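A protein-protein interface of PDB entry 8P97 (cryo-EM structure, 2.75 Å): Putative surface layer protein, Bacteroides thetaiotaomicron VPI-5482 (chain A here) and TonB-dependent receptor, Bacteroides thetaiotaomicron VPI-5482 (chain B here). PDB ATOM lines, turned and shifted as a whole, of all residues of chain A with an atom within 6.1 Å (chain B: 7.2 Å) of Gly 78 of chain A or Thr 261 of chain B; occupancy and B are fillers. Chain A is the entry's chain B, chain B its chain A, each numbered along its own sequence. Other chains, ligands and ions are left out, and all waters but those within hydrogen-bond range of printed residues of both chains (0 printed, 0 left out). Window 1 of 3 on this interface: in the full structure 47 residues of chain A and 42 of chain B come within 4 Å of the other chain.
The side-chain carboxylate (OD2) of Asp 197 of chain B is in salt-bridge range of the side-chain amino group (NZ) of Lys 76 of chain A, at 3.3 Å.
The backbone carbonyl oxygen (O) of Thr 261 of chain B is in hydrogen-bond range of the side-chain hydroxyl (OG) of Ser 98 of chain A, 2.8 Å away.
O of Ser 98 of chain A sits at hydrogen-bond distance from N of Gln 263 of chain B, at 3.4 Å.
The backbone carbonyl oxygen of Tyr 49 of chain A lies within hydrogen-bond range of the side-chain hydroxyl of Ser 661 of chain B.
The backbone NH of Asp 197 of chain B lies within hydrogen-bond range of the side-chain amide oxygen of Asn 195 of chain B (3.0 Å).
The backbone carbonyl oxygen (O) of Ser 661 of chain B sits at hydrogen-bond distance from the backbone NH (N) of Thr 260 of chain B (3.2 Å).
N of Tyr 49 of chain A is in hydrogen-bond range of OD1 of Asp 79 of chain A.
The backbone NH (N) of Gly 50 of chain A is in hydrogen-bond range of the side-chain carboxylate (OD1) of Asp 79 of chain A, at 2.6 Å.
N of Asp 79 of chain A lies within hydrogen-bond range of OG of Ser 98 of chain A (3.3 Å).
The backbone carbonyl oxygen (O) of Val 100 of chain A sits at hydrogen-bond distance from the backbone NH (N) of Val 95 of chain A, at 2.9 Å.
Among the printed residues, pairs that only touch across the chains: Lys 76 of chain A with Ser 661 of chain B (3.6 Å), Val 100 of chain A with Gln 263 of chain B (3.6 Å), Lys 76 of chain A with Thr 261 of chain B (3.6 Å), Gly 78 of chain A with Thr 261 of chain B (3.8 Å) and Gly 50 of chain A with Ser 661 of chain B (3.8 Å).
Of the 15 printed residues of chain B, 4 touch a printed residue of chain A.
Of the 16 printed residues of chain A, 6 touch a printed residue of chain B.
Along chain A the printed residues that touch a printed residue of chain B span positions 49 to 100.
Among the printed residues, 9 pairs touch across the chains.
Among the printed residues, Asp or Glu carboxylates within 4 Å of a Lys or Arg side-chain nitrogen of the other chain: Lys 76 of chain A with Asp 197 of chain B (3.3 Å).
Gly 78 of chain A touches one residue of chain B.
Of chain A, only Lys 76 (3.6 Å), Gly 78 (3.8 Å) and Ser 98 (2.8 Å) come within 4 Å of Thr 261 of chain B.
Printed residues of chain B within 4 Å of Val 100 of chain A: Gln 263.
Of the printed residues of chain A, Ser 661 of chain B touches Tyr 49, Gly 50 and Lys 76.
Asn 51 of chain A touches none of the printed residues of chain B.
The nearest residue of chain B that does not touch Gly 78 of chain A is Ser 661 of chain B (6.0 Å).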
ATOM      1  N   TYR A  49     -26.771 -11.071 -17.898  1.00  0.00           N
ATOM      2  CA  TYR A  49     -25.680 -11.869 -18.440  1.00  0.00           C
ATOM      3  C   TYR A  49     -25.294 -13.062 -17.586  1.00  0.00           C
ATOM      4  O   TYR A  49     -24.741 -14.024 -18.126  1.00  0.00           O
ATOM      5  CB  TYR A  49     -24.407 -11.035 -18.673  1.00  0.00           C
ATOM      6  CG  TYR A  49     -24.486 -10.010 -19.777  1.00  0.00           C
ATOM      7  CD1 TYR A  49     -25.507 -10.035 -20.707  1.00  0.00           C
ATOM      8  CD2 TYR A  49     -23.479  -9.073 -19.946  1.00  0.00           C
ATOM      9  CE1 TYR A  49     -25.565  -9.110 -21.727  1.00  0.00           C
ATOM     10  CE2 TYR A  49     -23.524  -8.149 -20.960  1.00  0.00           C
ATOM     11  CZ  TYR A  49     -24.567  -8.172 -21.850  1.00  0.00           C
ATOM     12  OH  TYR A  49     -24.614  -7.252 -22.869  1.00  0.00           O
ATOM     13  N   GLY A  50     -25.568 -13.040 -16.288  1.00  0.00           N
ATOM     14  CA  GLY A  50     -25.180 -14.147 -15.439  1.00  0.00           C
ATOM     15  C   GLY A  50     -23.682 -14.312 -15.311  1.00  0.00           C
ATOM     16  O   GLY A  50     -23.177 -15.438 -15.315  1.00  0.00           O
ATOM     17  N   ASN A  51     -22.955 -13.198 -15.203  1.00  0.00           N
ATOM     18  CA  ASN A  51     -21.515 -13.230 -14.969  1.00  0.00           C
ATOM     19  C   ASN A  51     -21.141 -12.655 -13.608  1.00  0.00           C
ATOM     20  O   ASN A  51     -20.005 -12.213 -13.420  1.00  0.00           O
ATOM     21  CB  ASN A  51     -20.761 -12.493 -16.077  1.00  0.00           C
ATOM     22  CG  ASN A  51     -21.351 -11.136 -16.385  1.00  0.00           C
ATOM     23  OD1 ASN A  51     -22.115 -10.582 -15.599  1.00  0.00           O
ATOM     24  ND2 ASN A  51     -20.985 -10.586 -17.534  1.00  0.00           N
ATOM     25  N   ALA A  52     -22.074 -12.637 -12.661  1.00  0.00           N
ATOM     26  CA  ALA A  52     -21.744 -12.240 -11.302  1.00  0.00           C
ATOM     27  C   ALA A  52     -20.780 -13.247 -10.695  1.00  0.00           C
ATOM     28  O   ALA A  52     -20.902 -14.453 -10.916  1.00  0.00           O
ATOM     29  CB  ALA A  52     -23.006 -12.140 -10.451  1.00  0.00           C
ATOM     30  N   THR A  53     -19.811 -12.751  -9.932  1.00  0.00           N
ATOM     31  CA  THR A  53     -18.757 -13.606  -9.410  1.00  0.00           C
ATOM     32  C   THR A  53     -18.251 -13.031  -8.094  1.00  0.00           C
ATOM     33  O   THR A  53     -18.478 -11.863  -7.772  1.00  0.00           O
ATOM     34  CB  THR A  53     -17.625 -13.760 -10.426  1.00  0.00           C
ATOM     35  OG1 THR A  53     -16.684 -14.727  -9.947  1.00  0.00           O
ATOM     36  CG2 THR A  53     -16.918 -12.438 -10.639  1.00  0.00           C
ATOM     37  N   LYS A  76     -21.973 -21.428 -11.731  1.00  0.00           N
ATOM     38  CA  LYS A  76     -21.950 -19.975 -11.715  1.00  0.00           C
ATOM     39  C   LYS A  76     -22.676 -19.426 -10.494  1.00  0.00           C
ATOM     40  O   LYS A  76     -23.589 -20.051  -9.952  1.00  0.00           O
ATOM     41  CB  LYS A  76     -22.577 -19.419 -12.990  1.00  0.00           C
ATOM     42  CG  LYS A  76     -21.759 -19.674 -14.238  1.00  0.00           C
ATOM     43  CD  LYS A  76     -22.414 -19.046 -15.446  1.00  0.00           C
ATOM     44  CE  LYS A  76     -21.615 -19.310 -16.703  1.00  0.00           C
ATOM     45  NZ  LYS A  76     -22.257 -18.696 -17.894  1.00  0.00           N
ATOM     46  N   LEU A  77     -22.251 -18.238 -10.061  1.00  0.00           N
ATOM     47  CA  LEU A  77     -22.833 -17.621  -8.874  1.00  0.00           C
ATOM     48  C   LEU A  77     -24.269 -17.182  -9.124  1.00  0.00           C
ATOM     49  O   LEU A  77     -25.154 -17.420  -8.294  1.00  0.00           O
ATOM     50  CB  LEU A  77     -21.981 -16.433  -8.431  1.00  0.00           C
ATOM     51  CG  LEU A  77     -22.462 -15.701  -7.180  1.00  0.00           C
ATOM     52  CD1 LEU A  77     -22.589 -16.664  -6.023  1.00  0.00           C
ATOM     53  CD2 LEU A  77     -21.534 -14.558  -6.828  1.00  0.00           C
ATOM     54  N   GLY A  78     -24.521 -16.534 -10.256  1.00  0.00           N
ATOM     55  CA  GLY A  78     -25.851 -16.043 -10.549  1.00  0.00           C
ATOM     56  C   GLY A  78     -25.863 -14.758 -11.349  1.00  0.00           C
ATOM     57  O   GLY A  78     -25.140 -14.635 -12.339  1.00  0.00           O
ATOM     58  N   ASP A  79     -26.673 -13.792 -10.921  1.00  0.00           N
ATOM     59  CA  ASP A  79     -26.867 -12.542 -11.649  1.00  0.00           C
ATOM     60  C   ASP A  79     -27.059 -11.407 -10.656  1.00  0.00           C
ATOM     61  O   ASP A  79     -27.996 -11.438  -9.855  1.00  0.00           O
ATOM     62  CB  ASP A  79     -28.075 -12.636 -12.583  1.00  0.00           C
ATOM     63  CG  ASP A  79     -27.956 -11.726 -13.785  1.00  0.00           C
ATOM     64  OD1 ASP A  79     -26.941 -11.803 -14.501  1.00  0.00           O
ATOM     65  OD2 ASP A  79     -28.882 -10.918 -14.006  1.00  0.00           O
ATOM     66  N   VAL A  80     -26.185 -10.403 -10.729  1.00  0.00           N
ATOM     67  CA  VAL A  80     -26.237  -9.218  -9.875  1.00  0.00           C
ATOM     68  C   VAL A  80     -26.129  -9.602  -8.406  1.00  0.00           C
ATOM     69  O   VAL A  80     -27.114  -9.542  -7.662  1.00  0.00           O
ATOM     70  CB  VAL A  80     -27.512  -8.395 -10.134  1.00  0.00           C
ATOM     71  CG1 VAL A  80     -27.426  -7.048  -9.435  1.00  0.00           C
ATOM     72  CG2 VAL A  80     -27.716  -8.206 -11.623  1.00  0.00           C
ATOM     73  N   ALA A  81     -24.938 -10.005  -7.976  1.00  0.00           N
ATOM     74  CA  ALA A  81     -24.694 -10.198  -6.556  1.00  0.00           C
ATOM     75  C   ALA A  81     -24.702  -8.851  -5.850  1.00  0.00           C
ATOM     76  O   ALA A  81     -24.120  -7.879  -6.335  1.00  0.00           O
ATOM     77  CB  ALA A  81     -23.360 -10.904  -6.338  1.00  0.00           C
ATOM     78  N   VAL A  95     -28.011 -12.922  -3.924  1.00  0.00           N
ATOM     79  CA  VAL A  95     -27.977 -12.673  -5.359  1.00  0.00           C
ATOM     80  C   VAL A  95     -29.326 -12.094  -5.752  1.00  0.00           C
ATOM     81  O   VAL A  95     -30.369 -12.713  -5.513  1.00  0.00           O
ATOM     82  CB  VAL A  95     -27.666 -13.952  -6.149  1.00  0.00           C
ATOM     83  CG1 VAL A  95     -27.397 -13.623  -7.598  1.00  0.00           C
ATOM     84  CG2 VAL A  95     -26.480 -14.668  -5.540  1.00  0.00           C
ATOM     85  N   ASN A  97     -30.793 -10.862  -8.911  1.00  0.00           N
ATOM     86  CA  ASN A  97     -31.539 -11.269 -10.093  1.00  0.00           C
ATOM     87  C   ASN A  97     -31.660 -12.780 -10.243  1.00  0.00           C
ATOM     88  O   ASN A  97     -32.052 -13.244 -11.318  1.00  0.00           O
ATOM     89  CB  ASN A  97     -30.890 -10.681 -11.346  1.00  0.00           C
ATOM     90  CG  ASN A  97     -31.896 -10.367 -12.428  1.00  0.00           C
ATOM     91  OD1 ASN A  97     -33.044 -10.034 -12.145  1.00  0.00           O
ATOM     92  ND2 ASN A  97     -31.470 -10.474 -13.679  1.00  0.00           N
ATOM     93  N   SER A  98     -31.336 -13.556  -9.212  1.00  0.00           N
ATOM     94  CA  SER A  98     -31.472 -15.003  -9.268  1.00  0.00           C
ATOM     95  C   SER A  98     -32.380 -15.566  -8.188  1.00  0.00           C
ATOM     96  O   SER A  98     -32.528 -16.790  -8.108  1.00  0.00           O
ATOM     97  CB  SER A  98     -30.097 -15.675  -9.177  1.00  0.00           C
ATOM     98  OG  SER A  98     -29.394 -15.549 -10.397  1.00  0.00           O
ATOM     99  N   VAL A 100     -32.098 -15.959  -5.001  1.00  0.00           N
ATOM    100  CA  VAL A 100     -31.376 -16.941  -4.201  1.00  0.00           C
ATOM    101  C   VAL A 100     -30.424 -16.225  -3.256  1.00  0.00           C
ATOM    102  O   VAL A 100     -29.899 -15.153  -3.566  1.00  0.00           O
ATOM    103  CB  VAL A 100     -30.614 -17.941  -5.102  1.00  0.00           C
ATOM    104  CG1 VAL A 100     -29.572 -17.222  -5.932  1.00  0.00           C
ATOM    105  CG2 VAL A 100     -29.985 -19.049  -4.280  1.00  0.00           C
ATOM    106  N   PHE A 102     -27.079 -17.629  -1.213  1.00  0.00           N
ATOM    107  CA  PHE A 102     -26.202 -18.779  -1.053  1.00  0.00           C
ATOM    108  C   PHE A 102     -25.538 -18.741   0.314  1.00  0.00           C
ATOM    109  O   PHE A 102     -25.130 -17.675   0.781  1.00  0.00           O
ATOM    110  CB  PHE A 102     -25.136 -18.798  -2.147  1.00  0.00           C
ATOM    111  CG  PHE A 102     -25.605 -19.384  -3.441  1.00  0.00           C
ATOM    112  CD1 PHE A 102     -25.832 -20.739  -3.558  1.00  0.00           C
ATOM    113  CD2 PHE A 102     -25.810 -18.580  -4.544  1.00  0.00           C
ATOM    114  CE1 PHE A 102     -26.259 -21.278  -4.747  1.00  0.00           C
ATOM    115  CE2 PHE A 102     -26.237 -19.116  -5.732  1.00  0.00           C
ATOM    116  CZ  PHE A 102     -26.461 -20.466  -5.835  1.00  0.00           C
ATOM    117  N   TYR B 193     -32.787 -29.486 -21.722  1.00  0.00           N
ATOM    118  CA  TYR B 193     -31.357 -29.278 -21.867  1.00  0.00           C
ATOM    119  C   TYR B 193     -30.661 -29.673 -20.575  1.00  0.00           C
ATOM    120  O   TYR B 193     -31.252 -29.622 -19.493  1.00  0.00           O
ATOM    121  CB  TYR B 193     -31.030 -27.821 -22.227  1.00  0.00           C
ATOM    122  CG  TYR B 193     -31.374 -26.821 -21.149  1.00  0.00           C
ATOM    123  CD1 TYR B 193     -32.636 -26.259 -21.081  1.00  0.00           C
ATOM    124  CD2 TYR B 193     -30.439 -26.438 -20.204  1.00  0.00           C
ATOM    125  CE1 TYR B 193     -32.957 -25.349 -20.104  1.00  0.00           C
ATOM    126  CE2 TYR B 193     -30.754 -25.528 -19.220  1.00  0.00           C
ATOM    127  CZ  TYR B 193     -32.015 -24.988 -19.176  1.00  0.00           C
ATOM    128  OH  TYR B 193     -32.340 -24.077 -18.200  1.00  0.00           O
ATOM    129  N   ASN B 195     -28.084 -28.859 -17.774  1.00  0.00           N
ATOM    130  CA  ASN B 195     -27.660 -27.578 -17.223  1.00  0.00           C
ATOM    131  C   ASN B 195     -26.295 -27.732 -16.560  1.00  0.00           C
ATOM    132  O   ASN B 195     -26.167 -28.408 -15.536  1.00  0.00           O
ATOM    133  CB  ASN B 195     -28.705 -27.067 -16.236  1.00  0.00           C
ATOM    134  CG  ASN B 195     -28.449 -25.649 -15.804  1.00  0.00           C
ATOM    135  OD1 ASN B 195     -27.455 -25.046 -16.192  1.00  0.00           O
ATOM    136  ND2 ASN B 195     -29.353 -25.100 -15.006  1.00  0.00           N
ATOM    137  N   ASP B 197     -24.506 -24.984 -15.565  1.00  0.00           N
ATOM    138  CA  ASP B 197     -24.246 -23.785 -14.782  1.00  0.00           C
ATOM    139  C   ASP B 197     -24.945 -23.798 -13.431  1.00  0.00           C
ATOM    140  O   ASP B 197     -24.876 -22.805 -12.701  1.00  0.00           O
ATOM    141  CB  ASP B 197     -24.666 -22.542 -15.566  1.00  0.00           C
ATOM    142  CG  ASP B 197     -23.791 -22.292 -16.774  1.00  0.00           C
ATOM    143  OD1 ASP B 197     -22.761 -22.980 -16.917  1.00  0.00           O
ATOM    144  OD2 ASP B 197     -24.135 -21.404 -17.580  1.00  0.00           O
ATOM    145  N   LYS B 198     -25.615 -24.890 -13.079  1.00  0.00           N
ATOM    146  CA  LYS B 198     -26.365 -24.958 -11.836  1.00  0.00           C
ATOM    147  C   LYS B 198     -26.343 -26.395 -11.341  1.00  0.00           C
ATOM    148  O   LYS B 198     -26.364 -27.329 -12.144  1.00  0.00           O
ATOM    149  CB  LYS B 198     -27.806 -24.474 -12.036  1.00  0.00           C
ATOM    150  CG  LYS B 198     -28.710 -24.667 -10.835  1.00  0.00           C
ATOM    151  CD  LYS B 198     -30.173 -24.660 -11.231  1.00  0.00           C
ATOM    152  CE  LYS B 198     -30.487 -23.530 -12.188  1.00  0.00           C
ATOM    153  NZ  LYS B 198     -31.953 -23.374 -12.382  1.00  0.00           N
ATOM    154  N   GLU B 217     -33.172 -29.727 -16.995  1.00  0.00           N
ATOM    155  CA  GLU B 217     -34.325 -28.851 -16.903  1.00  0.00           C
ATOM    156  C   GLU B 217     -34.995 -28.710 -18.263  1.00  0.00           C
ATOM    157  O   GLU B 217     -34.641 -29.374 -19.238  1.00  0.00           O
ATOM    158  CB  GLU B 217     -33.921 -27.477 -16.370  1.00  0.00           C
ATOM    159  CG  GLU B 217     -33.360 -27.478 -14.967  1.00  0.00           C
ATOM    160  CD  GLU B 217     -32.632 -26.192 -14.643  1.00  0.00           C
ATOM    161  OE1 GLU B 217     -31.581 -25.933 -15.262  1.00  0.00           O
ATOM    162  OE2 GLU B 217     -33.110 -25.439 -13.772  1.00  0.00           O
ATOM    163  N   ARG B 220     -37.978 -22.404 -19.727  1.00  0.00           N
ATOM    164  CA  ARG B 220     -39.123 -21.894 -18.991  1.00  0.00           C
ATOM    165  C   ARG B 220     -39.446 -20.477 -19.438  1.00  0.00           C
ATOM    166  O   ARG B 220     -38.550 -19.697 -19.774  1.00  0.00           O
ATOM    167  CB  ARG B 220     -38.865 -21.915 -17.485  1.00  0.00           C
ATOM    168  CG  ARG B 220     -38.757 -23.309 -16.903  1.00  0.00           C
ATOM    169  CD  ARG B 220     -38.726 -23.270 -15.391  1.00  0.00           C
ATOM    170  NE  ARG B 220     -37.558 -22.556 -14.891  1.00  0.00           N
ATOM    171  CZ  ARG B 220     -36.379 -23.117 -14.669  1.00  0.00           C
ATOM    172  NH1 ARG B 220     -36.173 -24.403 -14.900  1.00  0.00           N
ATOM    173  NH2 ARG B 220     -35.382 -22.370 -14.204  1.00  0.00           N
ATOM    174  N   LEU B 258     -36.253 -17.644 -19.054  1.00  0.00           N
ATOM    175  CA  LEU B 258     -35.432 -17.531 -17.861  1.00  0.00           C
ATOM    176  C   LEU B 258     -33.976 -17.824 -18.193  1.00  0.00           C
ATOM    177  O   LEU B 258     -33.668 -18.527 -19.158  1.00  0.00           O
ATOM    178  CB  LEU B 258     -35.918 -18.491 -16.777  1.00  0.00           C
ATOM    179  CG  LEU B 258     -37.297 -18.210 -16.186  1.00  0.00           C
ATOM    180  CD1 LEU B 258     -37.550 -19.109 -14.994  1.00  0.00           C
ATOM    181  CD2 LEU B 258     -37.424 -16.751 -15.797  1.00  0.00           C
ATOM    182  N   LEU B 259     -33.079 -17.278 -17.380  1.00  0.00           N
ATOM    183  CA  LEU B 259     -31.660 -17.507 -17.585  1.00  0.00           C
ATOM    184  C   LEU B 259     -31.256 -18.889 -17.088  1.00  0.00           C
ATOM    185  O   LEU B 259     -31.986 -19.559 -16.354  1.00  0.00           O
ATOM    186  CB  LEU B 259     -30.829 -16.442 -16.873  1.00  0.00           C
ATOM    187  CG  LEU B 259     -30.921 -15.018 -17.411  1.00  0.00           C
ATOM    188  CD1 LEU B 259     -30.177 -14.070 -16.495  1.00  0.00           C
ATOM    189  CD2 LEU B 259     -30.357 -14.953 -18.810  1.00  0.00           C
ATOM    190  N   THR B 260     -30.066 -19.315 -17.509  1.00  0.00           N
ATOM    191  CA  THR B 260     -29.533 -20.594 -17.058  1.00  0.00           C
ATOM    192  C   THR B 260     -29.293 -20.591 -15.555  1.00  0.00           C
ATOM    193  O   THR B 260     -29.585 -21.578 -14.869  1.00  0.00           O
ATOM    194  CB  THR B 260     -28.239 -20.909 -17.806  1.00  0.00           C
ATOM    195  OG1 THR B 260     -28.499 -20.959 -19.212  1.00  0.00           O
ATOM    196  CG2 THR B 260     -27.697 -22.234 -17.375  1.00  0.00           C
ATOM    197  N   THR B 261     -28.766 -19.490 -15.023  1.00  0.00           N
ATOM    198  CA  THR B 261     -28.445 -19.389 -13.600  1.00  0.00           C
ATOM    199  C   THR B 261     -29.597 -18.707 -12.861  1.00  0.00           C
ATOM    200  O   THR B 261     -29.471 -17.618 -12.301  1.00  0.00           O
ATOM    201  CB  THR B 261     -27.141 -18.633 -13.403  1.00  0.00           C
ATOM    202  OG1 THR B 261     -27.290 -17.299 -13.901  1.00  0.00           O
ATOM    203  CG2 THR B 261     -26.020 -19.314 -14.157  1.00  0.00           C
ATOM    204  N   ASP B 262     -30.741 -19.382 -12.872  1.00  0.00           N
ATOM    205  CA  ASP B 262     -31.936 -18.912 -12.187  1.00  0.00           C
ATOM    206  C   ASP B 262     -32.414 -20.014 -11.256  1.00  0.00           C
ATOM    207  O   ASP B 262     -32.660 -21.138 -11.700  1.00  0.00           O
ATOM    208  CB  ASP B 262     -33.024 -18.530 -13.188  1.00  0.00           C
ATOM    209  CG  ASP B 262     -34.140 -17.742 -12.556  1.00  0.00           C
ATOM    210  OD1 ASP B 262     -34.952 -18.350 -11.834  1.00  0.00           O
ATOM    211  OD2 ASP B 262     -34.208 -16.516 -12.782  1.00  0.00           O
ATOM    212  N   GLN B 263     -32.555 -19.689  -9.975  1.00  0.00           N
ATOM    213  CA  GLN B 263     -32.644 -20.692  -8.924  1.00  0.00           C
ATOM    214  C   GLN B 263     -34.084 -20.949  -8.512  1.00  0.00           C
ATOM    215  O   GLN B 263     -34.904 -20.030  -8.457  1.00  0.00           O
ATOM    216  CB  GLN B 263     -31.836 -20.259  -7.702  1.00  0.00           C
ATOM    217  CG  GLN B 263     -30.363 -20.077  -7.980  1.00  0.00           C
ATOM    218  CD  GLN B 263     -29.712 -21.339  -8.477  1.00  0.00           C
ATOM    219  OE1 GLN B 263     -29.313 -21.433  -9.635  1.00  0.00           O
ATOM    220  NE2 GLN B 263     -29.615 -22.328  -7.607  1.00  0.00           N
ATOM    221  N   SER B 661     -25.439 -17.522 -20.722  1.00  0.00           N
ATOM    222  CA  SER B 661     -26.516 -17.924 -19.815  1.00  0.00           C
ATOM    223  C   SER B 661     -27.868 -17.992 -20.523  1.00  0.00           C
ATOM    224  O   SER B 661     -28.899 -17.619 -19.963  1.00  0.00           O
ATOM    225  CB  SER B 661     -26.589 -16.993 -18.605  1.00  0.00           C
ATOM    226  OG  SER B 661     -25.550 -17.275 -17.685  1.00  0.00           O
ATOM    227  N   ARG B 662     -27.868 -18.480 -21.760  1.00  0.00           N
ATOM    228  CA  ARG B 662     -29.091 -18.649 -22.544  1.00  0.00           C
ATOM    229  C   ARG B 662     -29.147 -20.069 -23.089  1.00  0.00           C
ATOM    230  O   ARG B 662     -28.525 -20.361 -24.125  1.00  0.00           O
ATOM    231  CB  ARG B 662     -29.163 -17.639 -23.679  1.00  0.00           C
ATOM    232  CG  ARG B 662     -29.302 -16.202 -23.232  1.00  0.00           C
ATOM    233  CD  ARG B 662     -30.677 -15.938 -22.666  1.00  0.00           C
ATOM    234  NE  ARG B 662     -30.870 -14.531 -22.347  1.00  0.00           N
ATOM    235  CZ  ARG B 662     -31.972 -14.030 -21.808  1.00  0.00           C
ATOM    236  NH1 ARG B 662     -33.006 -14.798 -21.512  1.00  0.00           N
ATOM    237  NH2 ARG B 662     -32.039 -12.725 -21.561  1.00  0.00           N
ATOM    238  N   PRO B 663     -29.876 -20.971 -22.435  1.00  0.00           N
ATOM    239  CA  PRO B 663     -29.898 -22.367 -22.881  1.00  0.00           C
ATOM    240  C   PRO B 663     -30.494 -22.494 -24.272  1.00  0.00           C
ATOM    241  O   PRO B 663     -31.407 -21.758 -24.648  1.00  0.00           O
ATOM    242  CB  PRO B 663     -30.780 -23.055 -21.836  1.00  0.00           C
ATOM    243  CG  PRO B 663     -31.659 -21.963 -21.339  1.00  0.00           C
ATOM    244  CD  PRO B 663     -30.794 -20.745 -21.309  1.00  0.00           C
